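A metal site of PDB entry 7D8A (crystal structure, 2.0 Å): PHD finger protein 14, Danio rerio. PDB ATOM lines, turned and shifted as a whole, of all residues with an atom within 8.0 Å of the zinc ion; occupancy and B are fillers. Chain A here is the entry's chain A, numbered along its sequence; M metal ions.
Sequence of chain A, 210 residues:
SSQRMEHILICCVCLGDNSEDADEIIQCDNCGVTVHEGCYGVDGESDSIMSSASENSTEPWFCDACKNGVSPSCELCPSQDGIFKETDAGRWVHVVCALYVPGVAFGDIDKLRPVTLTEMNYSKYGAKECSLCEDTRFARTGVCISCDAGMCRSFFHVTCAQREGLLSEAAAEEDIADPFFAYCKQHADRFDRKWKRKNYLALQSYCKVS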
ATOM      1  N   LEU A  76     -10.780 -28.415  27.042  1.00  0.00           N
ATOM      2  CA  LEU A  76     -10.064 -27.283  26.457  1.00  0.00           C
ATOM      3  C   LEU A  76     -10.234 -25.968  27.218  1.00  0.00           C
ATOM      4  O   LEU A  76      -9.645 -24.967  26.800  1.00  0.00           O
ATOM      5  CB  LEU A  76     -10.517 -27.079  24.994  1.00  0.00           C
ATOM      6  CG  LEU A  76     -10.304 -28.267  24.038  1.00  0.00           C
ATOM      7  CD1 LEU A  76     -10.835 -27.963  22.634  1.00  0.00           C
ATOM      8  CD2 LEU A  76      -8.840 -28.648  23.966  1.00  0.00           C
ATOM      9  N   CYS A  77     -10.958 -25.953  28.334  1.00  0.00           N
ATOM     10  CA  CYS A  77     -11.178 -24.707  29.073  1.00  0.00           C
ATOM     11  C   CYS A  77     -11.806 -25.025  30.428  1.00  0.00           C
ATOM     12  O   CYS A  77     -12.255 -26.152  30.637  1.00  0.00           O
ATOM     13  CB  CYS A  77     -12.076 -23.751  28.273  1.00  0.00           C
ATOM     14  SG  CYS A  77     -13.862 -24.101  28.367  1.00  0.00           S
ATOM     15  N   PRO A  78     -11.855 -24.077  31.373  1.00  0.00           N
ATOM     16  CA  PRO A  78     -12.402 -24.392  32.701  1.00  0.00           C
ATOM     17  C   PRO A  78     -13.877 -24.093  32.899  1.00  0.00           C
ATOM     18  O   PRO A  78     -14.366 -24.242  34.026  1.00  0.00           O
ATOM     19  CB  PRO A  78     -11.566 -23.486  33.612  1.00  0.00           C
ATOM     20  CG  PRO A  78     -11.354 -22.246  32.764  1.00  0.00           C
ATOM     21  CD  PRO A  78     -11.211 -22.758  31.340  1.00  0.00           C
ATOM     22  N   SER A  79     -14.617 -23.664  31.868  1.00  0.00           N
ATOM     23  CA  SER A  79     -16.015 -23.311  32.053  1.00  0.00           C
ATOM     24  C   SER A  79     -16.911 -24.538  32.070  1.00  0.00           C
ATOM     25  O   SER A  79     -16.677 -25.511  31.349  1.00  0.00           O
ATOM     26  CB  SER A  79     -16.506 -22.385  30.943  1.00  0.00           C
ATOM     27  OG  SER A  79     -17.923 -22.281  30.969  1.00  0.00           O
ATOM     28  N   GLU A 129      -1.058 -18.755  29.290  1.00  0.00           N
ATOM     29  CA  GLU A 129      -1.881 -18.277  30.389  1.00  0.00           C
ATOM     30  C   GLU A 129      -3.050 -17.486  29.822  1.00  0.00           C
ATOM     31  O   GLU A 129      -2.862 -16.603  28.983  1.00  0.00           O
ATOM     32  CB  GLU A 129      -1.056 -17.401  31.326  1.00  0.00           C
ATOM     33  CG  GLU A 129      -1.878 -16.841  32.458  1.00  0.00           C
ATOM     34  CD  GLU A 129      -1.033 -16.050  33.430  1.00  0.00           C
ATOM     35  OE1 GLU A 129       0.200 -16.292  33.487  1.00  0.00           O
ATOM     36  OE2 GLU A 129      -1.590 -15.195  34.134  1.00  0.00           O
ATOM     37  N   CYS A 130      -4.259 -17.835  30.267  1.00  0.00           N
ATOM     38  CA  CYS A 130      -5.448 -17.113  29.796  1.00  0.00           C
ATOM     39  C   CYS A 130      -5.463 -15.713  30.409  1.00  0.00           C
ATOM     40  O   CYS A 130      -5.485 -15.563  31.632  1.00  0.00           O
ATOM     41  CB  CYS A 130      -6.710 -17.872  30.185  1.00  0.00           C
ATOM     42  SG  CYS A 130      -8.295 -16.986  29.844  1.00  0.00           S
ATOM     43  N   SER A 131      -5.457 -14.679  29.556  1.00  0.00           N
ATOM     44  CA  SER A 131      -5.410 -13.320  30.107  1.00  0.00           C
ATOM     45  C   SER A 131      -6.778 -12.811  30.566  1.00  0.00           C
ATOM     46  O   SER A 131      -6.843 -11.727  31.144  1.00  0.00           O
ATOM     47  CB  SER A 131      -4.820 -12.347  29.061  1.00  0.00           C
ATOM     48  OG  SER A 131      -5.632 -12.297  27.883  1.00  0.00           O
ATOM     49  N   LEU A 132      -7.853 -13.552  30.339  1.00  0.00           N
ATOM     50  CA  LEU A 132      -9.212 -13.127  30.683  1.00  0.00           C
ATOM     51  C   LEU A 132      -9.847 -13.935  31.795  1.00  0.00           C
ATOM     52  O   LEU A 132     -10.981 -13.636  32.166  1.00  0.00           O
ATOM     53  CB  LEU A 132     -10.111 -13.208  29.445  1.00  0.00           C
ATOM     54  CG  LEU A 132      -9.588 -12.358  28.286  1.00  0.00           C
ATOM     55  CD1 LEU A 132     -10.446 -12.553  27.050  1.00  0.00           C
ATOM     56  CD2 LEU A 132      -9.568 -10.893  28.729  1.00  0.00           C
ATOM     57  N   CYS A 133      -9.178 -14.980  32.315  1.00  0.00           N
ATOM     58  CA  CYS A 133      -9.764 -15.783  33.383  1.00  0.00           C
ATOM     59  C   CYS A 133     -10.062 -14.924  34.606  1.00  0.00           C
ATOM     60  O   CYS A 133      -9.206 -14.194  35.098  1.00  0.00           O
ATOM     61  CB  CYS A 133      -8.817 -16.926  33.763  1.00  0.00           C
ATOM     62  SG  CYS A 133      -9.316 -18.556  33.176  1.00  0.00           S
ATOM     63  N   GLU A 134     -11.294 -15.020  35.097  1.00  0.00           N
ATOM     64  CA  GLU A 134     -11.635 -14.320  36.328  1.00  0.00           C
ATOM     65  C   GLU A 134     -11.131 -15.070  37.565  1.00  0.00           C
ATOM     66  O   GLU A 134     -10.763 -14.440  38.557  1.00  0.00           O
ATOM     67  CB  GLU A 134     -13.146 -14.097  36.398  1.00  0.00           C
ATOM     68  CG  GLU A 134     -13.673 -13.222  35.261  1.00  0.00           C
ATOM     69  CD  GLU A 134     -15.172 -13.001  35.304  1.00  0.00           C
ATOM     70  OE1 GLU A 134     -15.905 -13.944  35.701  1.00  0.00           O
ATOM     71  OE2 GLU A 134     -15.627 -11.903  34.939  1.00  0.00           O
ATOM     72  N   ASP A 135     -11.081 -16.406  37.509  1.00  0.00           N
ATOM     73  CA  ASP A 135     -10.488 -17.201  38.584  1.00  0.00           C
ATOM     74  C   ASP A 135      -9.087 -17.591  38.133  1.00  0.00           C
ATOM     75  O   ASP A 135      -8.908 -18.451  37.272  1.00  0.00           O
ATOM     76  CB  ASP A 135     -11.348 -18.433  38.882  1.00  0.00           C
ATOM     77  CG  ASP A 135     -10.985 -19.100  40.207  1.00  0.00           C
ATOM     78  OD1 ASP A 135      -9.834 -18.968  40.668  1.00  0.00           O
ATOM     79  OD2 ASP A 135     -11.877 -19.754  40.778  1.00  0.00           O
ATOM     80  N   PHE A 138      -7.432 -21.121  37.308  1.00  0.00           N
ATOM     81  CA  PHE A 138      -7.705 -21.896  36.117  1.00  0.00           C
ATOM     82  C   PHE A 138      -7.105 -21.274  34.876  1.00  0.00           C
ATOM     83  O   PHE A 138      -7.361 -21.743  33.768  1.00  0.00           O
ATOM     84  CB  PHE A 138      -9.224 -22.064  35.935  1.00  0.00           C
ATOM     85  CG  PHE A 138      -9.916 -22.687  37.108  1.00  0.00           C
ATOM     86  CD1 PHE A 138      -9.977 -24.066  37.235  1.00  0.00           C
ATOM     87  CD2 PHE A 138     -10.508 -21.905  38.081  1.00  0.00           C
ATOM     88  CE1 PHE A 138     -10.622 -24.657  38.332  1.00  0.00           C
ATOM     89  CE2 PHE A 138     -11.148 -22.483  39.175  1.00  0.00           C
ATOM     90  CZ  PHE A 138     -11.201 -23.858  39.299  1.00  0.00           C
ATOM     91  N   ALA A 139      -6.304 -20.211  35.033  1.00  0.00           N
ATOM     92  CA  ALA A 139      -5.760 -19.525  33.863  1.00  0.00           C
ATOM     93  C   ALA A 139      -4.774 -20.379  33.082  1.00  0.00           C
ATOM     94  O   ALA A 139      -4.492 -20.074  31.920  1.00  0.00           O
ATOM     95  CB  ALA A 139      -5.079 -18.220  34.287  1.00  0.00           C
ATOM     96  N   ARG A 140      -4.232 -21.432  33.682  1.00  0.00           N
ATOM     97  CA  ARG A 140      -3.334 -22.329  32.953  1.00  0.00           C
ATOM     98  C   ARG A 140      -3.895 -23.750  32.881  1.00  0.00           C
ATOM     99  O   ARG A 140      -3.142 -24.715  32.834  1.00  0.00           O
ATOM    100  CB  ARG A 140      -1.942 -22.312  33.589  1.00  0.00           C
ATOM    101  CG  ARG A 140      -1.457 -20.891  33.806  1.00  0.00           C
ATOM    102  CD  ARG A 140       0.030 -20.789  33.749  1.00  0.00           C
ATOM    103  NE  ARG A 140       0.517 -21.321  32.485  1.00  0.00           N
ATOM    104  CZ  ARG A 140       1.225 -20.625  31.603  1.00  0.00           C
ATOM    105  NH1 ARG A 140       1.624 -21.206  30.489  1.00  0.00           N
ATOM    106  NH2 ARG A 140       1.553 -19.368  31.858  1.00  0.00           N
ATOM    107  N   THR A 141      -5.209 -23.887  32.891  1.00  0.00           N
ATOM    108  CA  THR A 141      -5.821 -25.138  32.491  1.00  0.00           C
ATOM    109  C   THR A 141      -6.180 -25.057  31.005  1.00  0.00           C
ATOM    110  O   THR A 141      -6.180 -23.986  30.409  1.00  0.00           O
ATOM    111  CB  THR A 141      -7.071 -25.431  33.318  1.00  0.00           C
ATOM    112  OG1 THR A 141      -8.040 -24.403  33.113  1.00  0.00           O
ATOM    113  CG2 THR A 141      -6.727 -25.483  34.800  1.00  0.00           C
ATOM    114  N   VAL A 143      -6.665 -25.040  26.968  1.00  0.00           N
ATOM    115  CA  VAL A 143      -5.922 -24.563  25.814  1.00  0.00           C
ATOM    116  C   VAL A 143      -6.417 -23.148  25.470  1.00  0.00           C
ATOM    117  O   VAL A 143      -7.624 -22.942  25.301  1.00  0.00           O
ATOM    118  CB  VAL A 143      -6.069 -25.526  24.607  1.00  0.00           C
ATOM    119  CG1 VAL A 143      -5.388 -24.986  23.329  1.00  0.00           C
ATOM    120  CG2 VAL A 143      -5.486 -26.911  24.966  1.00  0.00           C
ATOM    121  N   CYS A 144      -5.500 -22.203  25.374  1.00  0.00           N
ATOM    122  CA  CYS A 144      -5.823 -20.837  24.940  1.00  0.00           C
ATOM    123  C   CYS A 144      -5.678 -20.683  23.431  1.00  0.00           C
ATOM    124  O   CYS A 144      -4.818 -21.310  22.810  1.00  0.00           O
ATOM    125  CB  CYS A 144      -4.924 -19.801  25.624  1.00  0.00           C
ATOM    126  SG  CYS A 144      -5.165 -19.719  27.365  1.00  0.00           S
ATOM    127  N   PHE A 155      -3.500 -14.055  24.771  1.00  0.00           N
ATOM    128  CA  PHE A 155      -4.019 -15.409  24.835  1.00  0.00           C
ATOM    129  C   PHE A 155      -5.229 -15.487  25.755  1.00  0.00           C
ATOM    130  O   PHE A 155      -5.275 -14.802  26.784  1.00  0.00           O
ATOM    131  CB  PHE A 155      -2.938 -16.402  25.319  1.00  0.00           C
ATOM    132  CG  PHE A 155      -1.621 -16.286  24.592  1.00  0.00           C
ATOM    133  CD1 PHE A 155      -1.511 -16.632  23.261  1.00  0.00           C
ATOM    134  CD2 PHE A 155      -0.485 -15.862  25.261  1.00  0.00           C
ATOM    135  CE1 PHE A 155      -0.305 -16.534  22.584  1.00  0.00           C
ATOM    136  CE2 PHE A 155       0.735 -15.751  24.600  1.00  0.00           C
ATOM    137  CZ  PHE A 155       0.824 -16.092  23.257  1.00  0.00           C
ATOM    138  N   PHE A 156      -6.216 -16.300  25.389  1.00  0.00           N
ATOM    139  CA  PHE A 156      -7.371 -16.518  26.239  1.00  0.00           C
ATOM    140  C   PHE A 156      -8.024 -17.846  25.879  1.00  0.00           C
ATOM    141  O   PHE A 156      -7.936 -18.312  24.745  1.00  0.00           O
ATOM    142  CB  PHE A 156      -8.401 -15.373  26.096  1.00  0.00           C
ATOM    143  CG  PHE A 156      -8.328 -14.663  24.779  1.00  0.00           C
ATOM    144  CD1 PHE A 156      -8.683 -15.320  23.605  1.00  0.00           C
ATOM    145  CD2 PHE A 156      -7.854 -13.365  24.692  1.00  0.00           C
ATOM    146  CE1 PHE A 156      -8.572 -14.678  22.381  1.00  0.00           C
ATOM    147  CE2 PHE A 156      -7.750 -12.704  23.471  1.00  0.00           C
ATOM    148  CZ  PHE A 156      -8.113 -13.356  22.312  1.00  0.00           C
ATOM    149  N   HIS A 157      -8.694 -18.429  26.877  1.00  0.00           N
ATOM    150  CA  HIS A 157      -9.636 -19.520  26.642  1.00  0.00           C
ATOM    151  C   HIS A 157     -10.715 -19.085  25.657  1.00  0.00           C
ATOM    152  O   HIS A 157     -11.104 -17.916  25.636  1.00  0.00           O
ATOM    153  CB  HIS A 157     -10.293 -19.949  27.955  1.00  0.00           C
ATOM    154  CG  HIS A 157      -9.349 -20.622  28.902  1.00  0.00           C
ATOM    155  ND1 HIS A 157      -9.104 -20.153  30.169  1.00  0.00           N
ATOM    156  CD2 HIS A 157      -8.599 -21.747  28.767  1.00  0.00           C
ATOM    157  CE1 HIS A 157      -8.241 -20.936  30.778  1.00  0.00           C
ATOM    158  NE2 HIS A 157      -7.918 -21.922  29.949  1.00  0.00           N
ATOM    159  N   VAL A 158     -11.195 -20.017  24.846  1.00  0.00           N
ATOM    160  CA  VAL A 158     -12.255 -19.677  23.884  1.00  0.00           C
ATOM    161  C   VAL A 158     -13.481 -19.154  24.619  1.00  0.00           C
ATOM    162  O   VAL A 158     -14.080 -18.141  24.243  1.00  0.00           O
ATOM    163  CB  VAL A 158     -12.599 -20.880  22.998  1.00  0.00           C
ATOM    164  CG1 VAL A 158     -13.806 -20.552  22.093  1.00  0.00           C
ATOM    165  CG2 VAL A 158     -11.401 -21.319  22.156  1.00  0.00           C
ATOM    166  N   THR A 159     -13.888 -19.856  25.682  1.00  0.00           N
ATOM    167  CA  THR A 159     -15.088 -19.442  26.415  1.00  0.00           C
ATOM    168  C   THR A 159     -14.864 -18.174  27.236  1.00  0.00           C
ATOM    169  O   THR A 159     -15.831 -17.449  27.511  1.00  0.00           O
ATOM    170  CB  THR A 159     -15.577 -20.596  27.291  1.00  0.00           C
ATOM    171  OG1 THR A 159     -14.470 -21.124  28.010  1.00  0.00           O
ATOM    172  CG2 THR A 159     -16.182 -21.750  26.427  1.00  0.00           C
ATOM    173  N   CYS A 160     -13.625 -17.880  27.636  1.00  0.00           N
ATOM    174  CA  CYS A 160     -13.368 -16.591  28.288  1.00  0.00           C
ATOM    175  C   CYS A 160     -13.438 -15.439  27.283  1.00  0.00           C
ATOM    176  O   CYS A 160     -13.969 -14.374  27.603  1.00  0.00           O
ATOM    177  CB  CYS A 160     -12.014 -16.593  29.007  1.00  0.00           C
ATOM    178  SG  CYS A 160     -11.950 -17.717  30.444  1.00  0.00           S
ATOM    179  N   ALA A 161     -12.955 -15.664  26.056  1.00  0.00           N
ATOM    180  CA  ALA A 161     -13.120 -14.659  25.007  1.00  0.00           C
ATOM    181  C   ALA A 161     -14.590 -14.481  24.628  1.00  0.00           C
ATOM    182  O   ALA A 161     -15.041 -13.353  24.405  1.00  0.00           O
ATOM    183  CB  ALA A 161     -12.301 -15.059  23.767  1.00  0.00           C
ATOM    184  N   ARG A 163     -17.319 -14.712  26.424  1.00  0.00           N
ATOM    185  CA  ARG A 163     -17.964 -13.867  27.422  1.00  0.00           C
ATOM    186  C   ARG A 163     -17.659 -12.391  27.195  1.00  0.00           C
ATOM    187  O   ARG A 163     -18.529 -11.532  27.350  1.00  0.00           O
ATOM    188  CB  ARG A 163     -17.508 -14.328  28.816  1.00  0.00           C
ATOM    189  CG  ARG A 163     -17.761 -13.394  29.954  1.00  0.00           C
ATOM    190  CD  ARG A 163     -16.907 -13.791  31.164  1.00  0.00           C
ATOM    191  NE  ARG A 163     -15.716 -12.947  31.305  1.00  0.00           N
ATOM    192  CZ  ARG A 163     -14.464 -13.400  31.428  1.00  0.00           C
ATOM    193  NH1 ARG A 163     -13.471 -12.517  31.540  1.00  0.00           N
ATOM    194  NH2 ARG A 163     -14.194 -14.699  31.448  1.00  0.00           N
HETATM  195 ZN    ZN M   1      -9.802 -18.226  30.881  1.00  0.00          ZN
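SG of Cys 144 is in hydrogen-bond range of N of His 157 (3.8 Å). A ring nitrogen (NE2) of His 157 is in hydrogen-bond range of the backbone carbonyl oxygen (O) of Thr 141. The backbone NH (N) of Leu 132 sits close to the side-chain sulfur (SG) of Cys 130, at 3.5 Å. The backbone NH (N) of Cys 130 lies within hydrogen-bond range of the backbone carbonyl oxygen (O) of Ala 139 (2.8 Å). SG of Cys 144 sits close to N of Cys 130, 3.6 Å away. SG of Cys 133 lies close to O of Phe 138 (3.8 Å).
ND1 of His 157 binds the zinc ion (2.2 Å). The side-chain sulfur (SG) of Cys 130 is bound to the zinc ion, 2.2 Å away. The zinc ion is bound by SG of Cys 160. The side-chain sulfur (SG) of Cys 133 is bound to the zinc ion, at 2.4 Å.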
